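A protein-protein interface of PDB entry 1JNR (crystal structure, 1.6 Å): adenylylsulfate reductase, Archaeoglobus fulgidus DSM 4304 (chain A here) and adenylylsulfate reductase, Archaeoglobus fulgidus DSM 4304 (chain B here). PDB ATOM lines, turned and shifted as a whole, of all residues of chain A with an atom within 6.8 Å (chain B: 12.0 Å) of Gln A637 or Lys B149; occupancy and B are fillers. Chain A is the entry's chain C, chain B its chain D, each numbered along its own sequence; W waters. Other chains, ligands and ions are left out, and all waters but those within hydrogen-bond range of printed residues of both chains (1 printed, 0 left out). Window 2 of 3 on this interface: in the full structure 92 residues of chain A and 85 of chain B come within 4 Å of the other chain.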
ATOM      1  N   THR A  97     -15.483  19.321 -25.078  1.00  0.00           N
ATOM      2  CA  THR A  97     -14.618  18.449 -24.287  1.00  0.00           C
ATOM      3  C   THR A  97     -15.306  18.045 -22.985  1.00  0.00           C
ATOM      4  O   THR A  97     -15.243  16.884 -22.580  1.00  0.00           O
ATOM      5  CB  THR A  97     -13.268  19.135 -23.980  1.00  0.00           C
ATOM      6  OG1 THR A  97     -12.522  19.263 -25.196  1.00  0.00           O
ATOM      7  CG2 THR A  97     -12.452  18.313 -22.989  1.00  0.00           C
ATOM      8  N   GLU A 106      -9.488  18.075 -29.528  1.00  0.00           N
ATOM      9  CA  GLU A 106      -9.712  19.506 -29.640  1.00  0.00           C
ATOM     10  C   GLU A 106      -9.185  20.141 -30.915  1.00  0.00           C
ATOM     11  O   GLU A 106      -9.688  21.183 -31.345  1.00  0.00           O
ATOM     12  CB  GLU A 106      -9.159  20.210 -28.394  1.00  0.00           C
ATOM     13  CG  GLU A 106      -9.837  19.726 -27.119  1.00  0.00           C
ATOM     14  CD  GLU A 106      -9.407  20.490 -25.881  1.00  0.00           C
ATOM     15  OE1 GLU A 106      -8.403  21.230 -25.952  1.00  0.00           O
ATOM     16  OE2 GLU A 106     -10.074  20.339 -24.836  1.00  0.00           O
ATOM     17  N   PRO A 414      -1.477  18.545 -32.355  1.00  0.00           N
ATOM     18  CA  PRO A 414      -0.206  18.395 -31.643  1.00  0.00           C
ATOM     19  C   PRO A 414       0.493  17.106 -32.071  1.00  0.00           C
ATOM     20  O   PRO A 414      -0.148  16.181 -32.570  1.00  0.00           O
ATOM     21  CB  PRO A 414      -0.640  18.364 -30.183  1.00  0.00           C
ATOM     22  CG  PRO A 414      -1.946  17.632 -30.255  1.00  0.00           C
ATOM     23  CD  PRO A 414      -2.619  18.265 -31.462  1.00  0.00           C
ATOM     24  N   TYR A 417      -0.886  13.597 -31.308  1.00  0.00           N
ATOM     25  CA  TYR A 417      -1.946  12.991 -32.114  1.00  0.00           C
ATOM     26  C   TYR A 417      -1.569  12.660 -33.556  1.00  0.00           C
ATOM     27  O   TYR A 417      -2.384  12.114 -34.293  1.00  0.00           O
ATOM     28  CB  TYR A 417      -3.159  13.924 -32.155  1.00  0.00           C
ATOM     29  CG  TYR A 417      -3.804  14.225 -30.819  1.00  0.00           C
ATOM     30  CD1 TYR A 417      -4.639  15.332 -30.675  1.00  0.00           C
ATOM     31  CD2 TYR A 417      -3.627  13.386 -29.716  1.00  0.00           C
ATOM     32  CE1 TYR A 417      -5.285  15.598 -29.476  1.00  0.00           C
ATOM     33  CE2 TYR A 417      -4.270  13.644 -28.507  1.00  0.00           C
ATOM     34  CZ  TYR A 417      -5.099  14.753 -28.397  1.00  0.00           C
ATOM     35  OH  TYR A 417      -5.753  15.015 -27.218  1.00  0.00           O
ATOM     36  N   LYS A 614      -7.788   8.604 -19.073  1.00  0.00           N
ATOM     37  CA  LYS A 614      -8.102   9.868 -19.728  1.00  0.00           C
ATOM     38  C   LYS A 614      -7.322   9.823 -21.039  1.00  0.00           C
ATOM     39  O   LYS A 614      -6.371  10.576 -21.264  1.00  0.00           O
ATOM     40  CB  LYS A 614      -7.669  11.061 -18.869  1.00  0.00           C
ATOM     41  CG  LYS A 614      -8.297  12.359 -19.333  1.00  0.00           C
ATOM     42  CD  LYS A 614      -7.899  13.537 -18.478  1.00  0.00           C
ATOM     43  CE  LYS A 614      -8.614  14.793 -18.953  1.00  0.00           C
ATOM     44  NZ  LYS A 614      -8.231  15.981 -18.147  1.00  0.00           N
ATOM     45  N   TYR A 635      -5.110  12.008 -23.785  1.00  0.00           N
ATOM     46  CA  TYR A 635      -5.718  13.263 -24.182  1.00  0.00           C
ATOM     47  C   TYR A 635      -4.781  14.383 -23.751  1.00  0.00           C
ATOM     48  O   TYR A 635      -4.153  14.311 -22.694  1.00  0.00           O
ATOM     49  CB  TYR A 635      -7.064  13.450 -23.467  1.00  0.00           C
ATOM     50  CG  TYR A 635      -7.523  14.898 -23.349  1.00  0.00           C
ATOM     51  CD1 TYR A 635      -8.342  15.478 -24.315  1.00  0.00           C
ATOM     52  CD2 TYR A 635      -7.118  15.691 -22.272  1.00  0.00           C
ATOM     53  CE1 TYR A 635      -8.748  16.814 -24.214  1.00  0.00           C
ATOM     54  CE2 TYR A 635      -7.513  17.026 -22.163  1.00  0.00           C
ATOM     55  CZ  TYR A 635      -8.329  17.581 -23.135  1.00  0.00           C
ATOM     56  OH  TYR A 635      -8.713  18.899 -23.029  1.00  0.00           O
ATOM     57  N   VAL A 636      -4.670  15.407 -24.584  1.00  0.00           N
ATOM     58  CA  VAL A 636      -3.874  16.577 -24.240  1.00  0.00           C
ATOM     59  C   VAL A 636      -4.754  17.759 -24.605  1.00  0.00           C
ATOM     60  O   VAL A 636      -5.451  17.729 -25.623  1.00  0.00           O
ATOM     61  CB  VAL A 636      -2.538  16.663 -25.028  1.00  0.00           C
ATOM     62  CG1 VAL A 636      -1.612  15.537 -24.603  1.00  0.00           C
ATOM     63  CG2 VAL A 636      -2.798  16.619 -26.517  1.00  0.00           C
ATOM     64  N   GLN A 637      -4.754  18.787 -23.766  1.00  0.00           N
ATOM     65  CA  GLN A 637      -5.563  19.961 -24.049  1.00  0.00           C
ATOM     66  C   GLN A 637      -4.834  20.790 -25.095  1.00  0.00           C
ATOM     67  O   GLN A 637      -3.702  21.219 -24.885  1.00  0.00           O
ATOM     68  CB  GLN A 637      -5.791  20.785 -22.783  1.00  0.00           C
ATOM     69  CG  GLN A 637      -6.871  21.838 -22.963  1.00  0.00           C
ATOM     70  CD  GLN A 637      -7.163  22.606 -21.695  1.00  0.00           C
ATOM     71  OE1 GLN A 637      -7.166  22.041 -20.603  1.00  0.00           O
ATOM     72  NE2 GLN A 637      -7.430  23.897 -21.834  1.00  0.00           N
ATOM     73  N   VAL A 638      -5.491  21.004 -26.227  1.00  0.00           N
ATOM     74  CA  VAL A 638      -4.909  21.752 -27.333  1.00  0.00           C
ATOM     75  C   VAL A 638      -5.277  23.233 -27.332  1.00  0.00           C
ATOM     76  O   VAL A 638      -4.451  24.093 -27.650  1.00  0.00           O
ATOM     77  CB  VAL A 638      -5.353  21.126 -28.677  1.00  0.00           C
ATOM     78  CG1 VAL A 638      -4.757  21.893 -29.842  1.00  0.00           C
ATOM     79  CG2 VAL A 638      -4.925  19.662 -28.731  1.00  0.00           C
ATOM     80  N   ILE A 639      -6.523  23.521 -26.978  1.00  0.00           N
ATOM     81  CA  ILE A 639      -7.026  24.883 -26.961  1.00  0.00           C
ATOM     82  C   ILE A 639      -7.029  25.464 -25.559  1.00  0.00           C
ATOM     83  O   ILE A 639      -7.239  24.751 -24.577  1.00  0.00           O
ATOM     84  CB  ILE A 639      -8.453  24.921 -27.547  1.00  0.00           C
ATOM     85  CG1 ILE A 639      -8.422  24.414 -28.990  1.00  0.00           C
ATOM     86  CG2 ILE A 639      -9.031  26.330 -27.481  1.00  0.00           C
ATOM     87  CD1 ILE A 639      -7.474  25.185 -29.902  1.00  0.00           C
ATOM     88  N   GLU A 640      -6.792  26.768 -25.478  1.00  0.00           N
ATOM     89  CA  GLU A 640      -6.761  27.460 -24.201  1.00  0.00           C
ATOM     90  C   GLU A 640      -8.154  27.672 -23.622  1.00  0.00           C
ATOM     91  O   GLU A 640      -9.001  28.320 -24.232  1.00  0.00           O
ATOM     92  CB  GLU A 640      -6.062  28.811 -24.357  1.00  0.00           C
ATOM     93  CG  GLU A 640      -6.074  29.671 -23.105  1.00  0.00           C
ATOM     94  CD  GLU A 640      -5.351  30.987 -23.304  1.00  0.00           C
ATOM     95  OE1 GLU A 640      -4.124  30.962 -23.535  1.00  0.00           O
ATOM     96  OE2 GLU A 640      -6.010  32.045 -23.236  1.00  0.00           O
ATOM     97  N   TRP A 641      -8.372  27.105 -22.442  1.00  0.00           N
ATOM     98  CA  TRP A 641      -9.630  27.232 -21.716  1.00  0.00           C
ATOM     99  C   TRP A 641      -9.449  26.628 -20.334  1.00  0.00           C
ATOM    100  O   TRP A 641      -8.569  25.790 -20.123  1.00  0.00           O
ATOM    101  CB  TRP A 641     -10.791  26.525 -22.439  1.00  0.00           C
ATOM    102  CG  TRP A 641     -10.669  25.024 -22.597  1.00  0.00           C
ATOM    103  CD1 TRP A 641     -10.229  24.349 -23.702  1.00  0.00           C
ATOM    104  CD2 TRP A 641     -11.046  24.020 -21.642  1.00  0.00           C
ATOM    105  NE1 TRP A 641     -10.315  22.991 -23.497  1.00  0.00           N
ATOM    106  CE2 TRP A 641     -10.811  22.760 -22.242  1.00  0.00           C
ATOM    107  CE3 TRP A 641     -11.560  24.062 -20.337  1.00  0.00           C
ATOM    108  CZ2 TRP A 641     -11.074  21.553 -21.582  1.00  0.00           C
ATOM    109  CZ3 TRP A 641     -11.823  22.860 -19.681  1.00  0.00           C
ATOM    110  CH2 TRP A 641     -11.577  21.622 -20.307  1.00  0.00           C
ATOM    111  N   SER A 642     -10.264  27.076 -19.389  1.00  0.00           N
ATOM    112  CA  SER A 642     -10.206  26.565 -18.030  1.00  0.00           C
ATOM    113  C   SER A 642     -11.631  26.351 -17.548  1.00  0.00           C
ATOM    114  O   SER A 642     -12.570  26.962 -18.059  1.00  0.00           O
ATOM    115  CB  SER A 642      -9.483  27.550 -17.111  1.00  0.00           C
ATOM    116  OG  SER A 642     -10.161  28.791 -17.061  1.00  0.00           O
ATOM    117  N   GLN B 145      -9.391  33.085 -35.468  1.00  0.00           N
ATOM    118  CA  GLN B 145      -8.267  32.544 -34.726  1.00  0.00           C
ATOM    119  C   GLN B 145      -8.789  31.888 -33.459  1.00  0.00           C
ATOM    120  O   GLN B 145      -9.804  32.312 -32.909  1.00  0.00           O
ATOM    121  CB  GLN B 145      -7.292  33.662 -34.351  1.00  0.00           C
ATOM    122  CG  GLN B 145      -6.638  34.335 -35.541  1.00  0.00           C
ATOM    123  CD  GLN B 145      -5.714  33.403 -36.292  1.00  0.00           C
ATOM    124  OE1 GLN B 145      -4.727  32.912 -35.743  1.00  0.00           O
ATOM    125  NE2 GLN B 145      -6.030  33.147 -37.556  1.00  0.00           N
ATOM    126  N   VAL B 146      -8.104  30.844 -33.014  1.00  0.00           N
ATOM    127  CA  VAL B 146      -8.475  30.150 -31.789  1.00  0.00           C
ATOM    128  C   VAL B 146      -7.200  30.041 -30.959  1.00  0.00           C
ATOM    129  O   VAL B 146      -6.155  29.624 -31.465  1.00  0.00           O
ATOM    130  CB  VAL B 146      -9.056  28.745 -32.085  1.00  0.00           C
ATOM    131  CG1 VAL B 146      -8.027  27.884 -32.792  1.00  0.00           C
ATOM    132  CG2 VAL B 146      -9.515  28.093 -30.787  1.00  0.00           C
ATOM    133  N   LYS B 147      -7.279  30.439 -29.692  1.00  0.00           N
ATOM    134  CA  LYS B 147      -6.113  30.406 -28.819  1.00  0.00           C
ATOM    135  C   LYS B 147      -5.671  29.012 -28.472  1.00  0.00           C
ATOM    136  O   LYS B 147      -6.435  28.216 -27.925  1.00  0.00           O
ATOM    137  CB  LYS B 147      -6.381  31.149 -27.516  1.00  0.00           C
ATOM    138  CG  LYS B 147      -6.802  32.599 -27.722  1.00  0.00           C
ATOM    139  CD  LYS B 147      -7.111  33.267 -26.382  1.00  0.00           C
ATOM    140  CE  LYS B 147      -7.599  34.700 -26.558  1.00  0.00           C
ATOM    141  NZ  LYS B 147      -8.860  34.754 -27.353  1.00  0.00           N
ATOM    142  N   LYS B 148      -4.419  28.723 -28.784  1.00  0.00           N
ATOM    143  CA  LYS B 148      -3.867  27.431 -28.472  1.00  0.00           C
ATOM    144  C   LYS B 148      -3.376  27.461 -27.059  1.00  0.00           C
ATOM    145  O   LYS B 148      -2.920  28.494 -26.561  1.00  0.00           O
ATOM    146  CB  LYS B 148      -2.736  27.103 -29.415  1.00  0.00           C
ATOM    147  CG  LYS B 148      -3.265  26.513 -30.670  1.00  0.00           C
ATOM    148  CD  LYS B 148      -2.167  26.251 -31.637  1.00  0.00           C
ATOM    149  CE  LYS B 148      -1.710  24.834 -31.521  1.00  0.00           C
ATOM    150  NZ  LYS B 148      -0.720  24.605 -32.587  1.00  0.00           N
ATOM    151  N   LYS B 149      -3.470  26.320 -26.400  1.00  0.00           N
ATOM    152  CA  LYS B 149      -3.043  26.273 -25.036  1.00  0.00           C
ATOM    153  C   LYS B 149      -1.528  26.344 -24.903  1.00  0.00           C
ATOM    154  O   LYS B 149      -0.799  25.586 -25.543  1.00  0.00           O
ATOM    155  CB  LYS B 149      -3.578  25.028 -24.349  1.00  0.00           C
ATOM    156  CG  LYS B 149      -3.485  25.276 -22.876  1.00  0.00           C
ATOM    157  CD  LYS B 149      -3.400  24.018 -22.114  1.00  0.00           C
ATOM    158  CE  LYS B 149      -3.193  24.359 -20.675  1.00  0.00           C
ATOM    159  NZ  LYS B 149      -2.477  23.240 -20.049  1.00  0.00           N
ATOM    160  N   ALA B 150      -1.066  27.265 -24.062  1.00  0.00           N
ATOM    161  CA  ALA B 150       0.360  27.466 -23.821  1.00  0.00           C
ATOM    162  C   ALA B 150       1.077  26.155 -23.511  1.00  0.00           C
ATOM    163  O   ALA B 150       1.303  25.877 -22.316  1.00  0.00           O
ATOM    164  CB  ALA B 150       0.557  28.453 -22.675  1.00  0.00           C
ATOM    165  OXT ALA B 150       1.391  25.416 -24.468  1.00  0.00           O
HETATM  166  O   HOH W   1      -1.791  23.760 -28.304  1.00  0.00           O
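Gln A637 touches Lys B149 (O to CB, 3.8 Å). Lys B148 touches Val A638. Val B146 touches Ile A639. CG2 of Ile A639 touches O of Lys B147, at 3.2 Å. Ile A639 touches Lys B149. Lys B148 touches Glu A640.
Hydrophobic or aromatic side chains of chain B that line the printed part of chain A: Val B146. Along chain A the printed residues that touch a printed residue of chain B span positions 637 to 640. Among the printed residues, 9 pairs touch across the chains.
Water W1 lies within hydrogen-bond range of the backbone carbonyl oxygen (O) of Val A638 (2.8 Å) and the backbone carbonyl oxygen (O) of Lys B149 (3.5 Å).
The side-chain amide nitrogen (NE2) of Gln A637 lies within hydrogen-bond range of the backbone carbonyl oxygen (O) of Ile A639, 2.9 Å away. N of Ile A639 lies within hydrogen-bond range of OE1 of Glu A106 (3.1 Å). The side-chain carboxylate (OE1) of Glu A106 lies within hydrogen-bond range of the backbone NH (N) of Val A638, at 2.9 Å. NE2 of Gln A637 is in hydrogen-bond range of O of Trp A641 (2.8 Å).
N of Glu A640 lies within hydrogen-bond range of O of Lys B147 (2.9 Å). The backbone carbonyl oxygen (O) of Val A638 lies within hydrogen-bond range of the backbone NH (N) of Lys B149 (2.7 Å). The backbone NH of Glu A640 sits close to the backbone NH of Lys B149.
No residue of chain B comes within 4 Å of Val A636. Gln A637 touches just one residue of chain B: Lys B149 (3.8 Å). Ile A639 touches three residues of chain B. Of chain B, only Lys B147, Lys B148 and Lys B149 come within 4 Å of Glu A640. No residue of chain B comes within 4 Å of Trp A641. Ser A642 touches none of the printed residues of chain B. Gln B145 touches none of the printed residues of chain A. Of the printed residues of chain A, Val B146 touches Ile A639 (3.7 Å). Printed residues of chain A within 4 Å of Lys B147: Ile A639 (3.2 Å) and Glu A640 (2.9 Å). Of the printed residues of chain A, Lys B148 touches Val A638 (3.5 Å) and Glu A640 (3.8 Å). Lys B149 touches just these residues of chain A: Gln A637 (3.8 Å), Val A638 (2.7 Å), Ile A639 (3.7 Å) and Glu A640 (3.5 Å). The nearest printed residue of chain B that does not touch Gln A637 is Ala B150 (6.6 Å).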
